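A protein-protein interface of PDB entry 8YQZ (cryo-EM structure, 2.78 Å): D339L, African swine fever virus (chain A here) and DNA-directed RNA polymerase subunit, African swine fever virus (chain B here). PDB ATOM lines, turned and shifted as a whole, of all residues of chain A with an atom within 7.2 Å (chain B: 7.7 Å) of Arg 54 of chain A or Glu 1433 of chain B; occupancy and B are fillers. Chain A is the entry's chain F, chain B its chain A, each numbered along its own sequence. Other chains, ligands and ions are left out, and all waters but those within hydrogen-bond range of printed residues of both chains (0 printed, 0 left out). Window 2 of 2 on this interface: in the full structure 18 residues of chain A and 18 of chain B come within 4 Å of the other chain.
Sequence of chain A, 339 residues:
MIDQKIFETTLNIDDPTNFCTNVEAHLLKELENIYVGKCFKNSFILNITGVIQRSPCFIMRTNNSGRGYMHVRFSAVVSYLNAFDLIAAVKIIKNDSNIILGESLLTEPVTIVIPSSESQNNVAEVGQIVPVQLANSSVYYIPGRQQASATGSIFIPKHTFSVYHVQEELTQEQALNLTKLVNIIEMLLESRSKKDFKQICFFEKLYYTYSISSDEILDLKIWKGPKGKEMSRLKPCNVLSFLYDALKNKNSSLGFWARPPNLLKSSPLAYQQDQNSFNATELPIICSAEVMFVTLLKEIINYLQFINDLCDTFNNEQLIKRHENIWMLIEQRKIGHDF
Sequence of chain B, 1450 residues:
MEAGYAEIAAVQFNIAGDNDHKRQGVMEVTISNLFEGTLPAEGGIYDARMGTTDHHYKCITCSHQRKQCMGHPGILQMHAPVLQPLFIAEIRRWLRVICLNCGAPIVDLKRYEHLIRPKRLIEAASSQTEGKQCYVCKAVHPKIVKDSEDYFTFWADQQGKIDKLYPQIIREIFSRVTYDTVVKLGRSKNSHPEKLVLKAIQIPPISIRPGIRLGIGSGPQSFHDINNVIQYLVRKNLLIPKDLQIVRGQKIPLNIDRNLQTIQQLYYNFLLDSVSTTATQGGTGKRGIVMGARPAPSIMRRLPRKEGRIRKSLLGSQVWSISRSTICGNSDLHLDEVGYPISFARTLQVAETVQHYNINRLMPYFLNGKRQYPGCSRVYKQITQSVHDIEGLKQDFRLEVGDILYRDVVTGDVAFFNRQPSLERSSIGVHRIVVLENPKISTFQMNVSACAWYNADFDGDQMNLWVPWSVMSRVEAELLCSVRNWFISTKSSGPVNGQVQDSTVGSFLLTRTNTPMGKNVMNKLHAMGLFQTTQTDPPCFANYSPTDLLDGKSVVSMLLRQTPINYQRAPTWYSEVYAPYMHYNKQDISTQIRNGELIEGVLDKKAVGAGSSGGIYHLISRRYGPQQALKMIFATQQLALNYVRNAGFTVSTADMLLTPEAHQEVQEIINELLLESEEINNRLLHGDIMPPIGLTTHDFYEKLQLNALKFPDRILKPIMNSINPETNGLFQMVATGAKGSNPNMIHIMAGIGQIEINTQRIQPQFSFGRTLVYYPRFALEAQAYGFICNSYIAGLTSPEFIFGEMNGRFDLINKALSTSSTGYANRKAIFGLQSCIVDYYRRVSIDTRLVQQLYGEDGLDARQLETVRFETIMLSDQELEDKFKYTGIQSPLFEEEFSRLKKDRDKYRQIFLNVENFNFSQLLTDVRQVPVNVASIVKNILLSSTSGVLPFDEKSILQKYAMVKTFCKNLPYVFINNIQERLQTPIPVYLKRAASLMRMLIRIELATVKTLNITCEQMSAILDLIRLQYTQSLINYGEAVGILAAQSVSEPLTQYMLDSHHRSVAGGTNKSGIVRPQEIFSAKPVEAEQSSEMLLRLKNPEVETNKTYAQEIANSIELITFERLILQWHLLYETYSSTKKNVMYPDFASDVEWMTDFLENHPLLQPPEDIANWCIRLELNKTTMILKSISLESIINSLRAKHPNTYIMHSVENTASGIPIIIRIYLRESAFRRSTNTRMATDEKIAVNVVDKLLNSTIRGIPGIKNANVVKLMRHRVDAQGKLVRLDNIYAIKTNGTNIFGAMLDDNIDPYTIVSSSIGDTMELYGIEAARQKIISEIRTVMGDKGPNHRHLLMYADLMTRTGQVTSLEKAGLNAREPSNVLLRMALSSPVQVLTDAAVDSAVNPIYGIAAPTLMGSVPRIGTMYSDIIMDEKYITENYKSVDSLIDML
The backbone NH (N) of Met 1431 of chain B sits at hydrogen-bond distance from the backbone carbonyl oxygen (O) of Cys 57 of chain A (3.2 Å).
The side-chain hydroxyl (OG1) of Thr 1437 of chain B sits at hydrogen-bond distance from the backbone carbonyl oxygen (O) of Thr 21 of chain A (2.8 Å).
The side-chain carboxylate of Glu 1433 of chain B lies within salt-bridge range of the guanidinium group of Arg 54 of chain A, at 2.6 Å.
Printed residues of chain A that touch a printed residue of chain B: Pro 16, Cys 20, Thr 21, Val 23, Arg 54, Cys 57 and Phe 58.
Printed residues of chain B that touch a printed residue of chain A: Ile 1430, Met 1431, Glu 1433, Ile 1436 and Thr 1437.
Hydrophobic or aromatic side chains of chain B that line the printed part of chain A: Ile 1430, Met 1431 and Ile 1436.
Among the printed residues, Asp or Glu carboxylates within 4 Å of a Lys or Arg side-chain nitrogen of the other chain: Arg 54 of chain A with Glu 1433 of chain B (2.6 Å).
Among the printed residues, pairs that only touch across the chains: Cys 57 of chain A with Ile 1430 of chain B (3.4 Å), Phe 58 of chain A with Ile 1430 of chain B (3.4 Å), Pro 16 of chain A with Met 1431 of chain B (3.5 Å), Cys 20 of chain A with Glu 1433 of chain B (3.7 Å), Cys 20 of chain A with Met 1431 of chain B (3.7 Å), Val 23 of chain A with Glu 1433 of chain B (3.7 Å), Cys 57 of chain A with Glu 1433 of chain B (3.8 Å), Thr 21 of chain A with Ile 1436 of chain B (3.9 Å) and Cys 20 of chain A with Ile 1436 of chain B (3.99 Å).
The backbone carbonyl oxygen of Pro 16 of chain A sits close to the side-chain sulfur of Cys 20 of chain A (3.5 Å).
Of the printed residues of chain B, Pro 16 of chain A touches Met 1431 (3.5 Å).
Printed residues of chain B within 4 Å of Cys 20 of chain A: Met 1431 (3.7 Å), Glu 1433 (3.7 Å) and Ile 1436 (3.99 Å).
Of the printed residues of chain B, Val 23 of chain A touches Glu 1433.
Arg 54 of chain A touches one residue of chain B.
Met 70 of chain A touches none of the printed residues of chain B.
Arg 73 of chain A touches none of the printed residues of chain B.
Of the printed residues of chain A, Ile 1430 of chain B touches Cys 57 (3.4 Å) and Phe 58 (3.4 Å).
Of chain A, only Cys 20 (3.7 Å), Val 23 (3.7 Å), Arg 54 (2.6 Å) and Cys 57 (3.8 Å) come within 4 Å of Glu 1433 of chain B.
Of the printed residues of chain A, Ile 1436 of chain B touches Cys 20 (3.99 Å) and Thr 21 (3.9 Å).
The nearest printed residue of chain B that does not touch Arg 54 of chain A is Met 1431 of chain B (7.7 Å).
The nearest residue of chain A that does not touch Glu 1433 of chain B is Pro 56 of chain A (4.4 Å).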
ATOM      1  N   PRO A  16      23.650  -8.181  28.283  1.00  0.00           N
ATOM      2  CA  PRO A  16      23.807  -9.285  27.322  1.00  0.00           C
ATOM      3  C   PRO A  16      25.228  -9.806  27.179  1.00  0.00           C
ATOM      4  O   PRO A  16      25.418 -11.010  26.973  1.00  0.00           O
ATOM      5  CB  PRO A  16      23.285  -8.671  26.019  1.00  0.00           C
ATOM      6  CG  PRO A  16      22.414  -7.562  26.446  1.00  0.00           C
ATOM      7  CD  PRO A  16      23.040  -6.999  27.661  1.00  0.00           C
ATOM      8  N   PHE A  19      25.714 -12.033  30.148  1.00  0.00           N
ATOM      9  CA  PHE A  19      24.788 -13.157  30.104  1.00  0.00           C
ATOM     10  C   PHE A  19      25.249 -14.206  29.106  1.00  0.00           C
ATOM     11  O   PHE A  19      25.152 -15.407  29.368  1.00  0.00           O
ATOM     12  CB  PHE A  19      23.389 -12.660  29.757  1.00  0.00           C
ATOM     13  CG  PHE A  19      22.320 -13.709  29.842  1.00  0.00           C
ATOM     14  CD1 PHE A  19      22.048 -14.533  28.766  1.00  0.00           C
ATOM     15  CD2 PHE A  19      21.554 -13.844  30.981  1.00  0.00           C
ATOM     16  CE1 PHE A  19      21.065 -15.484  28.840  1.00  0.00           C
ATOM     17  CE2 PHE A  19      20.565 -14.789  31.050  1.00  0.00           C
ATOM     18  CZ  PHE A  19      20.326 -15.609  29.980  1.00  0.00           C
ATOM     19  N   CYS A  20      25.761 -13.774  27.959  1.00  0.00           N
ATOM     20  CA  CYS A  20      26.161 -14.713  26.922  1.00  0.00           C
ATOM     21  C   CYS A  20      27.509 -15.372  27.188  1.00  0.00           C
ATOM     22  O   CYS A  20      28.022 -16.059  26.303  1.00  0.00           O
ATOM     23  CB  CYS A  20      26.173 -14.011  25.562  1.00  0.00           C
ATOM     24  SG  CYS A  20      24.535 -13.692  24.894  1.00  0.00           S
ATOM     25  N   THR A  21      28.107 -15.166  28.361  1.00  0.00           N
ATOM     26  CA  THR A  21      29.301 -15.926  28.724  1.00  0.00           C
ATOM     27  C   THR A  21      28.965 -17.360  29.116  1.00  0.00           C
ATOM     28  O   THR A  21      29.772 -18.265  28.891  1.00  0.00           O
ATOM     29  CB  THR A  21      30.050 -15.226  29.856  1.00  0.00           C
ATOM     30  OG1 THR A  21      29.129 -14.879  30.894  1.00  0.00           O
ATOM     31  CG2 THR A  21      30.745 -13.981  29.358  1.00  0.00           C
ATOM     32  N   VAL A  23      25.233 -19.194  28.806  1.00  0.00           N
ATOM     33  CA  VAL A  23      23.813 -18.957  28.573  1.00  0.00           C
ATOM     34  C   VAL A  23      22.958 -19.913  29.390  1.00  0.00           C
ATOM     35  O   VAL A  23      21.951 -19.511  29.978  1.00  0.00           O
ATOM     36  CB  VAL A  23      23.496 -19.052  27.071  1.00  0.00           C
ATOM     37  CG1 VAL A  23      22.052 -18.705  26.822  1.00  0.00           C
ATOM     38  CG2 VAL A  23      24.397 -18.128  26.291  1.00  0.00           C
ATOM     39  N   GLU A  24      23.330 -21.188  29.431  1.00  0.00           N
ATOM     40  CA  GLU A  24      22.497 -22.186  30.096  1.00  0.00           C
ATOM     41  C   GLU A  24      22.407 -21.931  31.599  1.00  0.00           C
ATOM     42  O   GLU A  24      21.315 -21.953  32.181  1.00  0.00           O
ATOM     43  CB  GLU A  24      23.051 -23.580  29.806  1.00  0.00           C
ATOM     44  CG  GLU A  24      24.574 -23.657  29.834  1.00  0.00           C
ATOM     45  CD  GLU A  24      25.224 -23.250  28.517  1.00  0.00           C
ATOM     46  OE1 GLU A  24      24.504 -22.779  27.612  1.00  0.00           O
ATOM     47  OE2 GLU A  24      26.459 -23.389  28.390  1.00  0.00           O
ATOM     48  N   LEU A  27      20.516 -18.676  32.334  1.00  0.00           N
ATOM     49  CA  LEU A  27      19.110 -18.894  32.023  1.00  0.00           C
ATOM     50  C   LEU A  27      18.406 -19.673  33.122  1.00  0.00           C
ATOM     51  O   LEU A  27      17.314 -19.289  33.558  1.00  0.00           O
ATOM     52  CB  LEU A  27      18.994 -19.627  30.692  1.00  0.00           C
ATOM     53  CG  LEU A  27      17.673 -19.527  29.945  1.00  0.00           C
ATOM     54  CD1 LEU A  27      17.394 -18.088  29.627  1.00  0.00           C
ATOM     55  CD2 LEU A  27      17.757 -20.339  28.684  1.00  0.00           C
ATOM     56  N   VAL A  51      15.462 -26.581  30.249  1.00  0.00           N
ATOM     57  CA  VAL A  51      15.093 -25.679  29.167  1.00  0.00           C
ATOM     58  C   VAL A  51      15.009 -26.498  27.888  1.00  0.00           C
ATOM     59  O   VAL A  51      16.029 -26.966  27.368  1.00  0.00           O
ATOM     60  CB  VAL A  51      16.086 -24.522  29.025  1.00  0.00           C
ATOM     61  CG1 VAL A  51      15.811 -23.735  27.759  1.00  0.00           C
ATOM     62  CG2 VAL A  51      15.990 -23.624  30.230  1.00  0.00           C
ATOM     63  N   ILE A  52      13.788 -26.668  27.386  1.00  0.00           N
ATOM     64  CA  ILE A  52      13.569 -27.464  26.184  1.00  0.00           C
ATOM     65  C   ILE A  52      14.103 -26.744  24.957  1.00  0.00           C
ATOM     66  O   ILE A  52      14.807 -27.337  24.134  1.00  0.00           O
ATOM     67  CB  ILE A  52      12.071 -27.774  26.032  1.00  0.00           C
ATOM     68  CG1 ILE A  52      11.582 -28.639  27.186  1.00  0.00           C
ATOM     69  CG2 ILE A  52      11.803 -28.439  24.706  1.00  0.00           C
ATOM     70  CD1 ILE A  52      10.104 -28.612  27.340  1.00  0.00           C
ATOM     71  N   GLN A  53      13.789 -25.458  24.819  1.00  0.00           N
ATOM     72  CA  GLN A  53      14.000 -24.746  23.568  1.00  0.00           C
ATOM     73  C   GLN A  53      14.164 -23.267  23.867  1.00  0.00           C
ATOM     74  O   GLN A  53      13.492 -22.741  24.756  1.00  0.00           O
ATOM     75  CB  GLN A  53      12.816 -24.979  22.636  1.00  0.00           C
ATOM     76  CG  GLN A  53      13.158 -25.106  21.184  1.00  0.00           C
ATOM     77  CD  GLN A  53      11.990 -25.618  20.386  1.00  0.00           C
ATOM     78  OE1 GLN A  53      10.930 -25.900  20.936  1.00  0.00           O
ATOM     79  NE2 GLN A  53      12.167 -25.727  19.080  1.00  0.00           N
ATOM     80  N   ARG A  54      15.049 -22.598  23.134  1.00  0.00           N
ATOM     81  CA  ARG A  54      15.313 -21.185  23.359  1.00  0.00           C
ATOM     82  C   ARG A  54      15.647 -20.510  22.038  1.00  0.00           C
ATOM     83  O   ARG A  54      15.969 -21.163  21.048  1.00  0.00           O
ATOM     84  CB  ARG A  54      16.455 -20.981  24.358  1.00  0.00           C
ATOM     85  CG  ARG A  54      17.817 -21.224  23.768  1.00  0.00           C
ATOM     86  CD  ARG A  54      18.910 -20.853  24.719  1.00  0.00           C
ATOM     87  NE  ARG A  54      20.226 -21.050  24.135  1.00  0.00           N
ATOM     88  CZ  ARG A  54      20.877 -20.137  23.431  1.00  0.00           C
ATOM     89  NH1 ARG A  54      20.356 -18.949  23.195  1.00  0.00           N
ATOM     90  NH2 ARG A  54      22.081 -20.424  22.951  1.00  0.00           N
ATOM     91  N   SER A  55      15.581 -19.190  22.033  1.00  0.00           N
ATOM     92  CA  SER A  55      15.946 -18.365  20.897  1.00  0.00           C
ATOM     93  C   SER A  55      17.321 -17.757  21.107  1.00  0.00           C
ATOM     94  O   SER A  55      17.911 -17.883  22.182  1.00  0.00           O
ATOM     95  CB  SER A  55      14.920 -17.251  20.697  1.00  0.00           C
ATOM     96  OG  SER A  55      15.166 -16.180  21.577  1.00  0.00           O
ATOM     97  N   PRO A  56      17.886 -17.116  20.084  1.00  0.00           N
ATOM     98  CA  PRO A  56      19.074 -16.284  20.308  1.00  0.00           C
ATOM     99  C   PRO A  56      18.769 -15.116  21.235  1.00  0.00           C
ATOM    100  O   PRO A  56      17.628 -14.874  21.623  1.00  0.00           O
ATOM    101  CB  PRO A  56      19.432 -15.796  18.904  1.00  0.00           C
ATOM    102  CG  PRO A  56      18.868 -16.807  18.011  1.00  0.00           C
ATOM    103  CD  PRO A  56      17.622 -17.303  18.648  1.00  0.00           C
ATOM    104  N   CYS A  57      19.815 -14.389  21.599  1.00  0.00           N
ATOM    105  CA  CYS A  57      19.647 -13.194  22.421  1.00  0.00           C
ATOM    106  C   CYS A  57      19.492 -11.993  21.494  1.00  0.00           C
ATOM    107  O   CYS A  57      20.462 -11.452  20.973  1.00  0.00           O
ATOM    108  CB  CYS A  57      20.817 -13.026  23.380  1.00  0.00           C
ATOM    109  SG  CYS A  57      20.628 -11.682  24.566  1.00  0.00           S
ATOM    110  N   PHE A  58      18.250 -11.588  21.268  1.00  0.00           N
ATOM    111  CA  PHE A  58      17.973 -10.419  20.452  1.00  0.00           C
ATOM    112  C   PHE A  58      18.181  -9.140  21.246  1.00  0.00           C
ATOM    113  O   PHE A  58      17.902  -9.076  22.440  1.00  0.00           O
ATOM    114  CB  PHE A  58      16.540 -10.446  19.933  1.00  0.00           C
ATOM    115  CG  PHE A  58      16.147 -11.725  19.260  1.00  0.00           C
ATOM    116  CD1 PHE A  58      16.659 -12.055  18.026  1.00  0.00           C
ATOM    117  CD2 PHE A  58      15.234 -12.571  19.840  1.00  0.00           C
ATOM    118  CE1 PHE A  58      16.293 -13.212  17.402  1.00  0.00           C
ATOM    119  CE2 PHE A  58      14.860 -13.724  19.213  1.00  0.00           C
ATOM    120  CZ  PHE A  58      15.391 -14.046  17.992  1.00  0.00           C
ATOM    121  N   MET A  70      15.124 -12.877  25.406  1.00  0.00           N
ATOM    122  CA  MET A  70      15.217 -14.259  24.966  1.00  0.00           C
ATOM    123  C   MET A  70      13.870 -14.926  25.153  1.00  0.00           C
ATOM    124  O   MET A  70      13.179 -14.656  26.135  1.00  0.00           O
ATOM    125  CB  MET A  70      16.287 -15.010  25.754  1.00  0.00           C
ATOM    126  CG  MET A  70      16.807 -16.236  25.071  1.00  0.00           C
ATOM    127  SD  MET A  70      18.054 -17.065  26.047  1.00  0.00           S
ATOM    128  CE  MET A  70      19.521 -16.505  25.211  1.00  0.00           C
ATOM    129  N   HIS A  71      13.497 -15.781  24.212  1.00  0.00           N
ATOM    130  CA  HIS A  71      12.322 -16.624  24.355  1.00  0.00           C
ATOM    131  C   HIS A  71      12.770 -17.989  24.851  1.00  0.00           C
ATOM    132  O   HIS A  71      13.716 -18.565  24.312  1.00  0.00           O
ATOM    133  CB  HIS A  71      11.575 -16.764  23.029  1.00  0.00           C
ATOM    134  CG  HIS A  71      11.234 -15.463  22.377  1.00  0.00           C
ATOM    135  ND1 HIS A  71      10.379 -14.546  22.943  1.00  0.00           N
ATOM    136  CD2 HIS A  71      11.622 -14.934  21.196  1.00  0.00           C
ATOM    137  CE1 HIS A  71      10.259 -13.507  22.139  1.00  0.00           C
ATOM    138  NE2 HIS A  71      11.002 -13.719  21.073  1.00  0.00           N
ATOM    139  N   VAL A  72      12.112 -18.493  25.889  1.00  0.00           N
ATOM    140  CA  VAL A  72      12.485 -19.752  26.522  1.00  0.00           C
ATOM    141  C   VAL A  72      11.264 -20.651  26.593  1.00  0.00           C
ATOM    142  O   VAL A  72      10.169 -20.196  26.940  1.00  0.00           O
ATOM    143  CB  VAL A  72      13.074 -19.535  27.927  1.00  0.00           C
ATOM    144  CG1 VAL A  72      13.679 -20.809  28.441  1.00  0.00           C
ATOM    145  CG2 VAL A  72      14.122 -18.458  27.901  1.00  0.00           C
ATOM    146  N   ARG A  73      11.451 -21.920  26.258  1.00  0.00           N
ATOM    147  CA  ARG A  73      10.452 -22.960  26.467  1.00  0.00           C
ATOM    148  C   ARG A  73      11.058 -23.963  27.438  1.00  0.00           C
ATOM    149  O   ARG A  73      11.998 -24.679  27.087  1.00  0.00           O
ATOM    150  CB  ARG A  73      10.067 -23.617  25.144  1.00  0.00           C
ATOM    151  CG  ARG A  73       8.836 -24.475  25.207  1.00  0.00           C
ATOM    152  CD  ARG A  73       8.713 -25.317  23.967  1.00  0.00           C
ATOM    153  NE  ARG A  73       7.661 -24.827  23.086  1.00  0.00           N
ATOM    154  CZ  ARG A  73       7.850 -24.432  21.835  1.00  0.00           C
ATOM    155  NH1 ARG A  73       9.044 -24.469  21.271  1.00  0.00           N
ATOM    156  NH2 ARG A  73       6.813 -23.997  21.127  1.00  0.00           N
ATOM    157  N   ILE B1430      21.822  -9.752  16.938  1.00  0.00           N
ATOM    158  CA  ILE B1430      21.854 -10.760  17.986  1.00  0.00           C
ATOM    159  C   ILE B1430      23.278 -10.869  18.507  1.00  0.00           C
ATOM    160  O   ILE B1430      24.240 -10.497  17.837  1.00  0.00           O
ATOM    161  CB  ILE B1430      21.339 -12.132  17.511  1.00  0.00           C
ATOM    162  CG1 ILE B1430      22.249 -12.704  16.435  1.00  0.00           C
ATOM    163  CG2 ILE B1430      19.926 -12.031  17.008  1.00  0.00           C
ATOM    164  CD1 ILE B1430      21.861 -14.068  15.993  1.00  0.00           C
ATOM    165  N   MET B1431      23.408 -11.377  19.724  1.00  0.00           N
ATOM    166  CA  MET B1431      24.706 -11.449  20.375  1.00  0.00           C
ATOM    167  C   MET B1431      25.443 -12.692  19.899  1.00  0.00           C
ATOM    168  O   MET B1431      24.838 -13.753  19.733  1.00  0.00           O
ATOM    169  CB  MET B1431      24.557 -11.457  21.894  1.00  0.00           C
ATOM    170  CG  MET B1431      23.747 -10.294  22.418  1.00  0.00           C
ATOM    171  SD  MET B1431      24.675  -8.808  22.806  1.00  0.00           S
ATOM    172  CE  MET B1431      26.217  -9.472  23.371  1.00  0.00           C
ATOM    173  N   ASP B1432      26.740 -12.548  19.662  1.00  0.00           N
ATOM    174  CA  ASP B1432      27.586 -13.628  19.157  1.00  0.00           C
ATOM    175  C   ASP B1432      28.060 -14.476  20.332  1.00  0.00           C
ATOM    176  O   ASP B1432      29.109 -14.230  20.923  1.00  0.00           O
ATOM    177  CB  ASP B1432      28.750 -13.046  18.376  1.00  0.00           C
ATOM    178  CG  ASP B1432      29.415 -14.051  17.484  1.00  0.00           C
ATOM    179  OD1 ASP B1432      29.079 -15.250  17.565  1.00  0.00           O
ATOM    180  OD2 ASP B1432      30.286 -13.643  16.697  1.00  0.00           O
ATOM    181  N   GLU B1433      27.271 -15.499  20.666  1.00  0.00           N
ATOM    182  CA  GLU B1433      27.546 -16.321  21.840  1.00  0.00           C
ATOM    183  C   GLU B1433      28.838 -17.110  21.692  1.00  0.00           C
ATOM    184  O   GLU B1433      29.622 -17.209  22.640  1.00  0.00           O
ATOM    185  CB  GLU B1433      26.381 -17.271  22.082  1.00  0.00           C
ATOM    186  CG  GLU B1433      25.297 -16.702  22.943  1.00  0.00           C
ATOM    187  CD  GLU B1433      23.922 -17.155  22.510  1.00  0.00           C
ATOM    188  OE1 GLU B1433      23.671 -18.376  22.505  1.00  0.00           O
ATOM    189  OE2 GLU B1433      23.088 -16.292  22.174  1.00  0.00           O
ATOM    190  N   LYS B1434      29.072 -17.692  20.521  1.00  0.00           N
ATOM    191  CA  LYS B1434      30.252 -18.517  20.310  1.00  0.00           C
ATOM    192  C   LYS B1434      31.542 -17.710  20.346  1.00  0.00           C
ATOM    193  O   LYS B1434      32.619 -18.290  20.491  1.00  0.00           O
ATOM    194  CB  LYS B1434      30.117 -19.248  18.977  1.00  0.00           C
ATOM    195  CG  LYS B1434      30.999 -20.461  18.800  1.00  0.00           C
ATOM    196  CD  LYS B1434      31.096 -20.819  17.327  1.00  0.00           C
ATOM    197  CE  LYS B1434      32.351 -21.614  17.015  1.00  0.00           C
ATOM    198  NZ  LYS B1434      32.049 -23.064  16.826  1.00  0.00           N
ATOM    199  N   TYR B1435      31.461 -16.394  20.195  1.00  0.00           N
ATOM    200  CA  TYR B1435      32.624 -15.520  20.235  1.00  0.00           C
ATOM    201  C   TYR B1435      32.837 -14.906  21.607  1.00  0.00           C
ATOM    202  O   TYR B1435      33.982 -14.681  22.007  1.00  0.00           O
ATOM    203  CB  TYR B1435      32.468 -14.411  19.193  1.00  0.00           C
ATOM    204  CG  TYR B1435      33.618 -13.438  19.100  1.00  0.00           C
ATOM    205  CD1 TYR B1435      34.771 -13.763  18.416  1.00  0.00           C
ATOM    206  CD2 TYR B1435      33.537 -12.186  19.678  1.00  0.00           C
ATOM    207  CE1 TYR B1435      35.809 -12.876  18.318  1.00  0.00           C
ATOM    208  CE2 TYR B1435      34.575 -11.296  19.587  1.00  0.00           C
ATOM    209  CZ  TYR B1435      35.705 -11.647  18.906  1.00  0.00           C
ATOM    210  OH  TYR B1435      36.741 -10.756  18.818  1.00  0.00           O
ATOM    211  N   ILE B1436      31.757 -14.602  22.320  1.00  0.00           N
ATOM    212  CA  ILE B1436      31.863 -14.056  23.665  1.00  0.00           C
ATOM    213  C   ILE B1436      32.297 -15.129  24.648  1.00  0.00           C
ATOM    214  O   ILE B1436      33.119 -14.879  25.532  1.00  0.00           O
ATOM    215  CB  ILE B1436      30.529 -13.421  24.078  1.00  0.00           C
ATOM    216  CG1 ILE B1436      30.248 -12.181  23.243  1.00  0.00           C
ATOM    217  CG2 ILE B1436      30.543 -13.056  25.541  1.00  0.00           C
ATOM    218  CD1 ILE B1436      28.842 -11.689  23.387  1.00  0.00           C
ATOM    219  N   THR B1437      31.745 -16.336  24.519  1.00  0.00           N
ATOM    220  CA  THR B1437      32.068 -17.406  25.452  1.00  0.00           C
ATOM    221  C   THR B1437      33.512 -17.861  25.322  1.00  0.00           C
ATOM    222  O   THR B1437      34.042 -18.475  26.252  1.00  0.00           O
ATOM    223  CB  THR B1437      31.126 -18.593  25.242  1.00  0.00           C
ATOM    224  OG1 THR B1437      30.916 -19.260  26.487  1.00  0.00           O
ATOM    225  CG2 THR B1437      31.714 -19.583  24.262  1.00  0.00           C
ATOM    226  N   GLU B1438      34.160 -17.563  24.203  1.00  0.00           N
ATOM    227  CA  GLU B1438      35.530 -17.971  23.960  1.00  0.00           C
ATOM    228  C   GLU B1438      36.528 -16.855  24.233  1.00  0.00           C
ATOM    229  O   GLU B1438      37.705 -17.136  24.474  1.00  0.00           O
ATOM    230  CB  GLU B1438      35.654 -18.487  22.524  1.00  0.00           C
ATOM    231  CG  GLU B1438      36.945 -18.179  21.818  1.00  0.00           C
ATOM    232  CD  GLU B1438      37.047 -18.884  20.489  1.00  0.00           C
ATOM    233  OE1 GLU B1438      35.992 -19.202  19.902  1.00  0.00           O
ATOM    234  OE2 GLU B1438      38.182 -19.130  20.032  1.00  0.00           O
ATOM    235  N   ASN B1439      36.079 -15.605  24.258  1.00  0.00           N
ATOM    236  CA  ASN B1439      36.959 -14.455  24.404  1.00  0.00           C
ATOM    237  C   ASN B1439      36.722 -13.648  25.667  1.00  0.00           C
ATOM    238  O   ASN B1439      37.651 -12.973  26.122  1.00  0.00           O
ATOM    239  CB  ASN B1439      36.800 -13.517  23.200  1.00  0.00           C
ATOM    240  CG  ASN B1439      37.347 -14.103  21.924  1.00  0.00           C
ATOM    241  OD1 ASN B1439      36.601 -14.612  21.096  1.00  0.00           O
ATOM    242  ND2 ASN B1439      38.653 -14.022  21.750  1.00  0.00           N
